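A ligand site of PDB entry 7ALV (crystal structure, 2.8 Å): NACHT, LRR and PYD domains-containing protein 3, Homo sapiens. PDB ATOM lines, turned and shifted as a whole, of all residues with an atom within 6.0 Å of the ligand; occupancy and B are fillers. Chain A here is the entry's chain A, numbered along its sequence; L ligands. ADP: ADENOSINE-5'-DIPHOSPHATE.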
ATOM      1  N   ILE A  22     -10.744  31.742  14.261  1.00  0.00           N
ATOM      2  CA  ILE A  22     -11.154  30.975  15.438  1.00  0.00           C
ATOM      3  C   ILE A  22     -11.143  31.832  16.739  1.00  0.00           C
ATOM      4  O   ILE A  22     -11.860  31.528  17.683  1.00  0.00           O
ATOM      5  CB  ILE A  22     -10.267  29.714  15.559  1.00  0.00           C
ATOM      6  N   ARG A  38      -9.481  26.077   9.072  1.00  0.00           N
ATOM      7  CA  ARG A  38      -9.171  24.918   9.883  1.00  0.00           C
ATOM      8  C   ARG A  38     -10.489  24.255  10.340  1.00  0.00           C
ATOM      9  O   ARG A  38     -10.420  23.130  10.852  1.00  0.00           O
ATOM     10  CB  ARG A  38      -8.312  25.296  11.107  1.00  0.00           C
ATOM     11  CG  ARG A  38      -7.205  24.281  11.479  1.00  0.00           C
ATOM     12  CD  ARG A  38      -6.624  24.578  12.860  1.00  0.00           C
ATOM     13  NE  ARG A  38      -5.189  24.870  12.843  1.00  0.00           N
ATOM     14  CZ  ARG A  38      -4.553  25.564  13.803  1.00  0.00           C
ATOM     15  NH1 ARG A  38      -5.232  26.050  14.840  1.00  0.00           N
ATOM     16  NH2 ARG A  38      -3.248  25.785  13.714  1.00  0.00           N
ATOM     17  N   TYR A  39     -11.677  24.928  10.185  1.00  0.00           N
ATOM     18  CA  TYR A  39     -12.975  24.372  10.584  1.00  0.00           C
ATOM     19  C   TYR A  39     -13.235  23.052   9.893  1.00  0.00           C
ATOM     20  O   TYR A  39     -13.308  22.977   8.664  1.00  0.00           O
ATOM     21  CB  TYR A  39     -14.170  25.344  10.389  1.00  0.00           C
ATOM     22  CG  TYR A  39     -15.501  24.693  10.741  1.00  0.00           C
ATOM     23  CD1 TYR A  39     -15.921  24.602  12.060  1.00  0.00           C
ATOM     24  CD2 TYR A  39     -16.291  24.093   9.772  1.00  0.00           C
ATOM     25  CE1 TYR A  39     -17.106  23.943  12.402  1.00  0.00           C
ATOM     26  CE2 TYR A  39     -17.468  23.423  10.099  1.00  0.00           C
ATOM     27  CZ  TYR A  39     -17.870  23.345  11.418  1.00  0.00           C
ATOM     28  OH  TYR A  39     -19.028  22.681  11.750  1.00  0.00           O
ATOM     29  N   THR A  40     -13.362  22.009  10.706  1.00  0.00           N
ATOM     30  CA  THR A  40     -13.654  20.650  10.282  1.00  0.00           C
ATOM     31  C   THR A  40     -15.069  20.335  10.764  1.00  0.00           C
ATOM     32  O   THR A  40     -15.395  20.606  11.911  1.00  0.00           O
ATOM     33  CB  THR A  40     -12.616  19.713  10.867  1.00  0.00           C
ATOM     34  OG1 THR A  40     -11.341  20.101  10.383  1.00  0.00           O
ATOM     35  CG2 THR A  40     -12.878  18.284  10.515  1.00  0.00           C
ATOM     36  N   ARG A  41     -15.928  19.794   9.890  1.00  0.00           N
ATOM     37  CA  ARG A  41     -17.323  19.515  10.243  1.00  0.00           C
ATOM     38  C   ARG A  41     -17.483  18.741  11.563  1.00  0.00           C
ATOM     39  O   ARG A  41     -16.693  17.849  11.864  1.00  0.00           O
ATOM     40  CB  ARG A  41     -18.029  18.800   9.079  1.00  0.00           C
ATOM     41  CG  ARG A  41     -19.511  18.505   9.346  1.00  0.00           C
ATOM     42  CD  ARG A  41     -19.932  17.133   8.827  1.00  0.00           C
ATOM     43  NE  ARG A  41     -19.921  17.072   7.360  1.00  0.00           N
ATOM     44  CZ  ARG A  41     -20.108  15.959   6.664  1.00  0.00           C
ATOM     45  NH1 ARG A  41     -20.326  14.803   7.283  1.00  0.00           N
ATOM     46  NH2 ARG A  41     -20.070  15.991   5.332  1.00  0.00           N
ATOM     47  N   LEU A  42     -18.458  19.141  12.377  1.00  0.00           N
ATOM     48  CA  LEU A  42     -18.714  18.465  13.637  1.00  0.00           C
ATOM     49  C   LEU A  42     -19.922  17.530  13.486  1.00  0.00           C
ATOM     50  O   LEU A  42     -20.785  17.777  12.632  1.00  0.00           O
ATOM     51  CB  LEU A  42     -18.953  19.486  14.759  1.00  0.00           C
ATOM     52  CG  LEU A  42     -17.752  20.352  15.132  1.00  0.00           C
ATOM     53  CD1 LEU A  42     -18.148  21.467  16.050  1.00  0.00           C
ATOM     54  CD2 LEU A  42     -16.692  19.525  15.786  1.00  0.00           C
ATOM     55  N   GLY A  97     -22.736  19.912  24.754  1.00  0.00           N
ATOM     56  CA  GLY A  97     -21.412  19.562  24.265  1.00  0.00           C
ATOM     57  C   GLY A  97     -20.347  19.621  25.335  1.00  0.00           C
ATOM     58  O   GLY A  97     -20.254  20.606  26.066  1.00  0.00           O
ATOM     59  N   ALA A  98     -19.525  18.558  25.451  1.00  0.00           N
ATOM     60  CA  ALA A  98     -18.467  18.509  26.469  1.00  0.00           C
ATOM     61  C   ALA A  98     -17.447  19.626  26.267  1.00  0.00           C
ATOM     62  O   ALA A  98     -17.308  20.126  25.151  1.00  0.00           O
ATOM     63  CB  ALA A  98     -17.772  17.158  26.423  1.00  0.00           C
ATOM     64  N   ALA A  99     -16.710  20.006  27.325  1.00  0.00           N
ATOM     65  CA  ALA A  99     -15.697  21.064  27.196  1.00  0.00           C
ATOM     66  C   ALA A  99     -14.642  20.675  26.158  1.00  0.00           C
ATOM     67  O   ALA A  99     -14.174  19.526  26.164  1.00  0.00           O
ATOM     68  CB  ALA A  99     -15.021  21.319  28.523  1.00  0.00           C
ATOM     69  N   GLY A 100     -14.366  21.561  25.224  1.00  0.00           N
ATOM     70  CA  GLY A 100     -13.423  21.290  24.157  1.00  0.00           C
ATOM     71  C   GLY A 100     -14.022  20.605  22.938  1.00  0.00           C
ATOM     72  O   GLY A 100     -13.283  20.297  21.998  1.00  0.00           O
ATOM     73  N   ILE A 101     -15.344  20.364  22.929  1.00  0.00           N
ATOM     74  CA  ILE A 101     -15.972  19.695  21.789  1.00  0.00           C
ATOM     75  C   ILE A 101     -16.145  20.624  20.588  1.00  0.00           C
ATOM     76  O   ILE A 101     -16.266  20.128  19.476  1.00  0.00           O
ATOM     77  CB  ILE A 101     -17.303  18.961  22.143  1.00  0.00           C
ATOM     78  CG1 ILE A 101     -17.522  17.725  21.251  1.00  0.00           C
ATOM     79  CG2 ILE A 101     -18.498  19.878  22.099  1.00  0.00           C
ATOM     80  CD1 ILE A 101     -16.573  16.543  21.482  1.00  0.00           C
ATOM     81  N   GLY A 102     -16.140  21.944  20.787  1.00  0.00           N
ATOM     82  CA  GLY A 102     -16.283  22.883  19.686  1.00  0.00           C
ATOM     83  C   GLY A 102     -17.520  23.766  19.669  1.00  0.00           C
ATOM     84  O   GLY A 102     -17.869  24.302  18.619  1.00  0.00           O
ATOM     85  N   LYS A 103     -18.173  23.948  20.824  1.00  0.00           N
ATOM     86  CA  LYS A 103     -19.373  24.779  20.975  1.00  0.00           C
ATOM     87  C   LYS A 103     -19.145  26.207  20.418  1.00  0.00           C
ATOM     88  O   LYS A 103     -19.873  26.683  19.550  1.00  0.00           O
ATOM     89  CB  LYS A 103     -19.763  24.851  22.462  1.00  0.00           C
ATOM     90  CG  LYS A 103     -20.780  23.843  22.932  1.00  0.00           C
ATOM     91  CD  LYS A 103     -20.304  23.098  24.142  1.00  0.00           C
ATOM     92  CE  LYS A 103     -19.927  23.981  25.302  1.00  0.00           C
ATOM     93  NZ  LYS A 103     -18.710  23.463  26.004  1.00  0.00           N
ATOM     94  N   THR A 104     -18.105  26.868  20.932  1.00  0.00           N
ATOM     95  CA  THR A 104     -17.710  28.226  20.594  1.00  0.00           C
ATOM     96  C   THR A 104     -17.269  28.315  19.145  1.00  0.00           C
ATOM     97  O   THR A 104     -17.632  29.267  18.479  1.00  0.00           O
ATOM     98  CB  THR A 104     -16.604  28.640  21.559  1.00  0.00           C
ATOM     99  OG1 THR A 104     -17.019  28.408  22.919  1.00  0.00           O
ATOM    100  CG2 THR A 104     -16.175  30.054  21.371  1.00  0.00           C
ATOM    101  N   ILE A 105     -16.551  27.307  18.619  1.00  0.00           N
ATOM    102  CA  ILE A 105     -16.123  27.316  17.215  1.00  0.00           C
ATOM    103  C   ILE A 105     -17.335  27.203  16.275  1.00  0.00           C
ATOM    104  O   ILE A 105     -17.457  27.992  15.345  1.00  0.00           O
ATOM    105  CB  ILE A 105     -15.031  26.260  16.921  1.00  0.00           C
ATOM    106  CG1 ILE A 105     -13.710  26.636  17.593  1.00  0.00           C
ATOM    107  CG2 ILE A 105     -14.846  26.045  15.423  1.00  0.00           C
ATOM    108  CD1 ILE A 105     -13.238  28.083  17.379  1.00  0.00           C
ATOM    109  N   LEU A 106     -18.251  26.272  16.565  1.00  0.00           N
ATOM    110  CA  LEU A 106     -19.462  26.095  15.783  1.00  0.00           C
ATOM    111  C   LEU A 106     -20.360  27.337  15.848  1.00  0.00           C
ATOM    112  O   LEU A 106     -21.037  27.652  14.864  1.00  0.00           O
ATOM    113  CB  LEU A 106     -20.235  24.876  16.292  1.00  0.00           C
ATOM    114  CG  LEU A 106     -21.520  24.581  15.574  1.00  0.00           C
ATOM    115  CD1 LEU A 106     -21.260  24.228  14.098  1.00  0.00           C
ATOM    116  CD2 LEU A 106     -22.286  23.546  16.303  1.00  0.00           C
ATOM    117  N   ASP A 173     -23.571  31.790  23.802  1.00  0.00           N
ATOM    118  CA  ASP A 173     -22.504  30.828  23.811  1.00  0.00           C
ATOM    119  C   ASP A 173     -21.872  30.577  25.182  1.00  0.00           C
ATOM    120  O   ASP A 173     -21.234  31.462  25.763  1.00  0.00           O
ATOM    121  CB  ASP A 173     -21.426  31.214  22.790  1.00  0.00           C
ATOM    122  CG  ASP A 173     -20.225  30.298  22.745  1.00  0.00           C
ATOM    123  OD1 ASP A 173     -20.409  29.044  22.877  1.00  0.00           O
ATOM    124  OD2 ASP A 173     -19.100  30.810  22.585  1.00  0.00           O
ATOM    125  N   PHE A 244     -15.560  15.113  16.391  1.00  0.00           N
ATOM    126  CA  PHE A 244     -15.051  14.499  15.183  1.00  0.00           C
ATOM    127  C   PHE A 244     -15.295  13.034  15.045  1.00  0.00           C
ATOM    128  O   PHE A 244     -15.105  12.287  15.995  1.00  0.00           O
ATOM    129  CB  PHE A 244     -13.549  14.743  15.035  1.00  0.00           C
ATOM    130  CG  PHE A 244     -13.152  16.191  14.848  1.00  0.00           C
ATOM    131  CD1 PHE A 244     -14.023  17.087  14.258  1.00  0.00           C
ATOM    132  CD2 PHE A 244     -11.913  16.637  15.239  1.00  0.00           C
ATOM    133  CE1 PHE A 244     -13.676  18.408  14.102  1.00  0.00           C
ATOM    134  CE2 PHE A 244     -11.550  17.967  15.059  1.00  0.00           C
ATOM    135  CZ  PHE A 244     -12.433  18.841  14.490  1.00  0.00           C
ATOM    136  N   TYR A 252      -8.784  16.769  10.368  1.00  0.00           N
ATOM    137  CA  TYR A 252      -8.187  17.791  11.227  1.00  0.00           C
ATOM    138  C   TYR A 252      -6.673  17.728  11.180  1.00  0.00           C
ATOM    139  O   TYR A 252      -6.030  18.757  10.973  1.00  0.00           O
ATOM    140  CB  TYR A 252      -8.690  17.688  12.680  1.00  0.00           C
ATOM    141  CG  TYR A 252      -8.141  18.816  13.523  1.00  0.00           C
ATOM    142  CD1 TYR A 252      -6.904  18.703  14.144  1.00  0.00           C
ATOM    143  CD2 TYR A 252      -8.828  20.014  13.646  1.00  0.00           C
ATOM    144  CE1 TYR A 252      -6.353  19.766  14.837  1.00  0.00           C
ATOM    145  CE2 TYR A 252      -8.293  21.068  14.363  1.00  0.00           C
ATOM    146  CZ  TYR A 252      -7.054  20.946  14.952  1.00  0.00           C
ATOM    147  OH  TYR A 252      -6.524  21.992  15.658  1.00  0.00           O
ATOM    148  N   PRO A 283     -12.297  17.865  19.539  1.00  0.00           N
ATOM    149  CA  PRO A 283     -11.419  18.716  18.725  1.00  0.00           C
ATOM    150  C   PRO A 283     -10.332  19.440  19.507  1.00  0.00           C
ATOM    151  O   PRO A 283      -9.214  19.586  18.984  1.00  0.00           O
ATOM    152  CB  PRO A 283     -12.398  19.674  18.041  1.00  0.00           C
ATOM    153  CG  PRO A 283     -13.700  18.912  18.028  1.00  0.00           C
ATOM    154  CD  PRO A 283     -13.713  18.224  19.355  1.00  0.00           C
ATOM    155  N   LEU A 284     -10.581  19.829  20.784  1.00  0.00           N
ATOM    156  CA  LEU A 284      -9.540  20.458  21.591  1.00  0.00           C
ATOM    157  C   LEU A 284      -8.373  19.478  21.777  1.00  0.00           C
ATOM    158  O   LEU A 284      -7.241  19.836  21.460  1.00  0.00           O
ATOM    159  CB  LEU A 284     -10.046  20.983  22.935  1.00  0.00           C
ATOM    160  CG  LEU A 284      -8.978  21.580  23.854  1.00  0.00           C
ATOM    161  CD1 LEU A 284      -8.254  22.727  23.224  1.00  0.00           C
ATOM    162  CD2 LEU A 284      -9.566  22.044  25.170  1.00  0.00           C
ATOM    163  N   TRP A 287      -6.314  19.418  18.749  1.00  0.00           N
ATOM    164  CA  TRP A 287      -5.462  20.605  18.701  1.00  0.00           C
ATOM    165  C   TRP A 287      -4.253  20.491  19.644  1.00  0.00           C
ATOM    166  O   TRP A 287      -3.143  20.893  19.287  1.00  0.00           O
ATOM    167  CB  TRP A 287      -6.283  21.871  19.010  1.00  0.00           C
ATOM    168  CG  TRP A 287      -5.444  23.111  19.024  1.00  0.00           C
ATOM    169  CD1 TRP A 287      -5.007  23.817  17.951  1.00  0.00           C
ATOM    170  CD2 TRP A 287      -4.805  23.691  20.175  1.00  0.00           C
ATOM    171  NE1 TRP A 287      -4.148  24.821  18.347  1.00  0.00           N
ATOM    172  CE2 TRP A 287      -4.008  24.767  19.719  1.00  0.00           C
ATOM    173  CE3 TRP A 287      -4.787  23.385  21.543  1.00  0.00           C
ATOM    174  CZ2 TRP A 287      -3.242  25.544  20.575  1.00  0.00           C
ATOM    175  CZ3 TRP A 287      -4.036  24.173  22.399  1.00  0.00           C
ATOM    176  CH2 TRP A 287      -3.295  25.258  21.908  1.00  0.00           C
ATOM    177  N   ILE A 392      -5.976  29.750  27.366  1.00  0.00           N
ATOM    178  CA  ILE A 392      -6.315  29.177  26.052  1.00  0.00           C
ATOM    179  C   ILE A 392      -7.631  28.409  26.087  1.00  0.00           C
ATOM    180  O   ILE A 392      -8.327  28.322  25.081  1.00  0.00           O
ATOM    181  CB  ILE A 392      -5.185  28.340  25.417  1.00  0.00           C
ATOM    182  CG1 ILE A 392      -4.345  27.570  26.466  1.00  0.00           C
ATOM    183  CG2 ILE A 392      -4.290  29.221  24.593  1.00  0.00           C
ATOM    184  CD1 ILE A 392      -3.543  26.454  25.844  1.00  0.00           C
ATOM    185  N   HIS A 393      -7.981  27.868  27.252  1.00  0.00           N
ATOM    186  CA  HIS A 393      -9.238  27.181  27.472  1.00  0.00           C
ATOM    187  C   HIS A 393      -9.456  27.100  28.964  1.00  0.00           C
ATOM    188  O   HIS A 393      -8.519  27.187  29.731  1.00  0.00           O
ATOM    189  CB  HIS A 393      -9.231  25.779  26.866  1.00  0.00           C
ATOM    190  CG  HIS A 393     -10.578  25.270  26.499  1.00  0.00           C
ATOM    191  ND1 HIS A 393     -11.316  24.461  27.343  1.00  0.00           N
ATOM    192  CD2 HIS A 393     -11.302  25.487  25.374  1.00  0.00           C
ATOM    193  CE1 HIS A 393     -12.459  24.214  26.718  1.00  0.00           C
ATOM    194  NE2 HIS A 393     -12.488  24.791  25.518  1.00  0.00           N
ATOM    195  N   MET A 394     -10.708  26.913  29.368  1.00  0.00           N
ATOM    196  CA  MET A 394     -11.035  26.771  30.780  1.00  0.00           C
ATOM    197  C   MET A 394     -10.542  25.421  31.328  1.00  0.00           C
ATOM    198  O   MET A 394     -10.176  25.378  32.496  1.00  0.00           O
ATOM    199  CB  MET A 394     -12.508  27.055  31.080  1.00  0.00           C
ATOM    200  CG  MET A 394     -13.448  26.483  30.043  1.00  0.00           C
ATOM    201  SD  MET A 394     -14.139  24.821  30.284  1.00  0.00           S
ATOM    202  CE  MET A 394     -15.691  24.990  29.171  1.00  0.00           C
HETATM  203  PB  ADP L   1     -16.000  24.602  23.878  1.00  0.00           P
HETATM  204  O1B ADP L   1     -15.214  24.483  25.230  1.00  0.00           O
HETATM  205  O2B ADP L   1     -17.091  23.586  23.773  1.00  0.00           O
HETATM  206  O3B ADP L   1     -16.429  26.087  23.792  1.00  0.00           O
HETATM  207  PA  ADP L   1     -14.299  25.291  21.634  1.00  0.00           P
HETATM  208  O1A ADP L   1     -13.904  26.542  22.476  1.00  0.00           O
HETATM  209  O2A ADP L   1     -15.235  25.691  20.568  1.00  0.00           O
HETATM  210  O3A ADP L   1     -15.029  24.307  22.647  1.00  0.00           O
HETATM  211  O5' ADP L   1     -12.957  24.572  21.044  1.00  0.00           O
HETATM  212  C5' ADP L   1     -11.615  24.942  21.419  1.00  0.00           C
HETATM  213  C4' ADP L   1     -10.625  24.452  20.400  1.00  0.00           C
HETATM  214  O4' ADP L   1     -11.189  23.317  19.709  1.00  0.00           O
HETATM  215  C3' ADP L   1     -10.228  25.455  19.323  1.00  0.00           C
HETATM  216  O3' ADP L   1      -9.073  26.181  19.725  1.00  0.00           O
HETATM  217  C2' ADP L   1      -9.960  24.576  18.087  1.00  0.00           C
HETATM  218  O2' ADP L   1      -8.611  24.332  17.698  1.00  0.00           O
HETATM  219  C1' ADP L   1     -10.751  23.288  18.372  1.00  0.00           C
HETATM  220  N9  ADP L   1     -11.922  23.149  17.534  1.00  0.00           N
HETATM  221  C8  ADP L   1     -13.217  23.070  17.976  1.00  0.00           C
HETATM  222  N7  ADP L   1     -14.087  22.840  17.026  1.00  0.00           N
HETATM  223  C5  ADP L   1     -13.323  22.763  15.872  1.00  0.00           C
HETATM  224  C6  ADP L   1     -13.637  22.512  14.532  1.00  0.00           C
HETATM  225  N6  ADP L   1     -14.859  22.171  14.133  1.00  0.00           N
HETATM  226  N1  ADP L   1     -12.635  22.537  13.628  1.00  0.00           N
HETATM  227  C2  ADP L   1     -11.395  22.780  14.059  1.00  0.00           C
HETATM  228  N3  ADP L   1     -10.959  22.983  15.298  1.00  0.00           N
HETATM  229  C4  ADP L   1     -11.977  22.965  16.178  1.00  0.00           C
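The side-chain hydroxyl (OG1) of Thr 40 is in hydrogen-bond range of the backbone carbonyl oxygen (O) of Arg 38, 3.2 Å away. OG1 of Thr 104 sits at hydrogen-bond distance from OD2 of Asp 173. The backbone carbonyl oxygen (O) of Gly 100 sits at hydrogen-bond distance from the backbone NH (N) of Leu 284 (3.0 Å). NZ of Lys 103 sits close to O of Gly 97, at 3.2 Å.
NZ of Lys 103 lies within salt-bridge range of O2B of the ligand, at 2.8 Å. OG1 of Thr 104 lies within hydrogen-bond range of O3B of the ligand, 2.5 Å away. An oxygen (O3A) of the ligand lies within hydrogen-bond range of the backbone NH (N) of Gly 102. O2A of the ligand is in hydrogen-bond range of N of Thr 104. The backbone NH of Gly 100 lies within hydrogen-bond range of an oxygen (O1B) of the ligand. N of Lys 103 is in hydrogen-bond range of O2B of the ligand (3.2 Å). N1 of the ligand sits at hydrogen-bond distance from N of Thr 40 (3.1 Å). O of Thr 40 is in hydrogen-bond range of N6 of the ligand (2.8 Å). A ring nitrogen (NE2) of His 393 sits at hydrogen-bond distance from an oxygen (O1B) of the ligand (2.8 Å). The backbone NH (N) of Ile 105 is in hydrogen-bond range of an oxygen (O2A) of the ligand (2.9 Å).
Arg 38 touches the ligand (O to C2, 3.4 Å). CE1 of Tyr 39 touches N6 of the ligand, at 3.3 Å. Leu 42 touches the ligand (CG to N6, 3.6 Å). Ala 98 touches the ligand (O to O2B, 3.7 Å). Ala 99 touches the ligand (C to O1B, 3.96 Å). Ile 101 touches the ligand. Phe 244 touches the ligand. CE2 of Tyr 252 touches N3 of the ligand, at 3.4 Å. CB of Pro 283 touches C8 of the ligand, 3.5 Å away. Leu 284 touches the ligand (N to O4', 3.7 Å). CB of Trp 287 touches O2' of the ligand (3.6 Å). Hydrophobic or aromatic side chains within 4 Å of the ligand: Tyr 39, Leu 42, Ile 105, Phe 244, Tyr 252, Pro 283, Trp 287 and His 393. The nearest printed residue that does not touch the ligand is Met 394 (4.002 Å).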
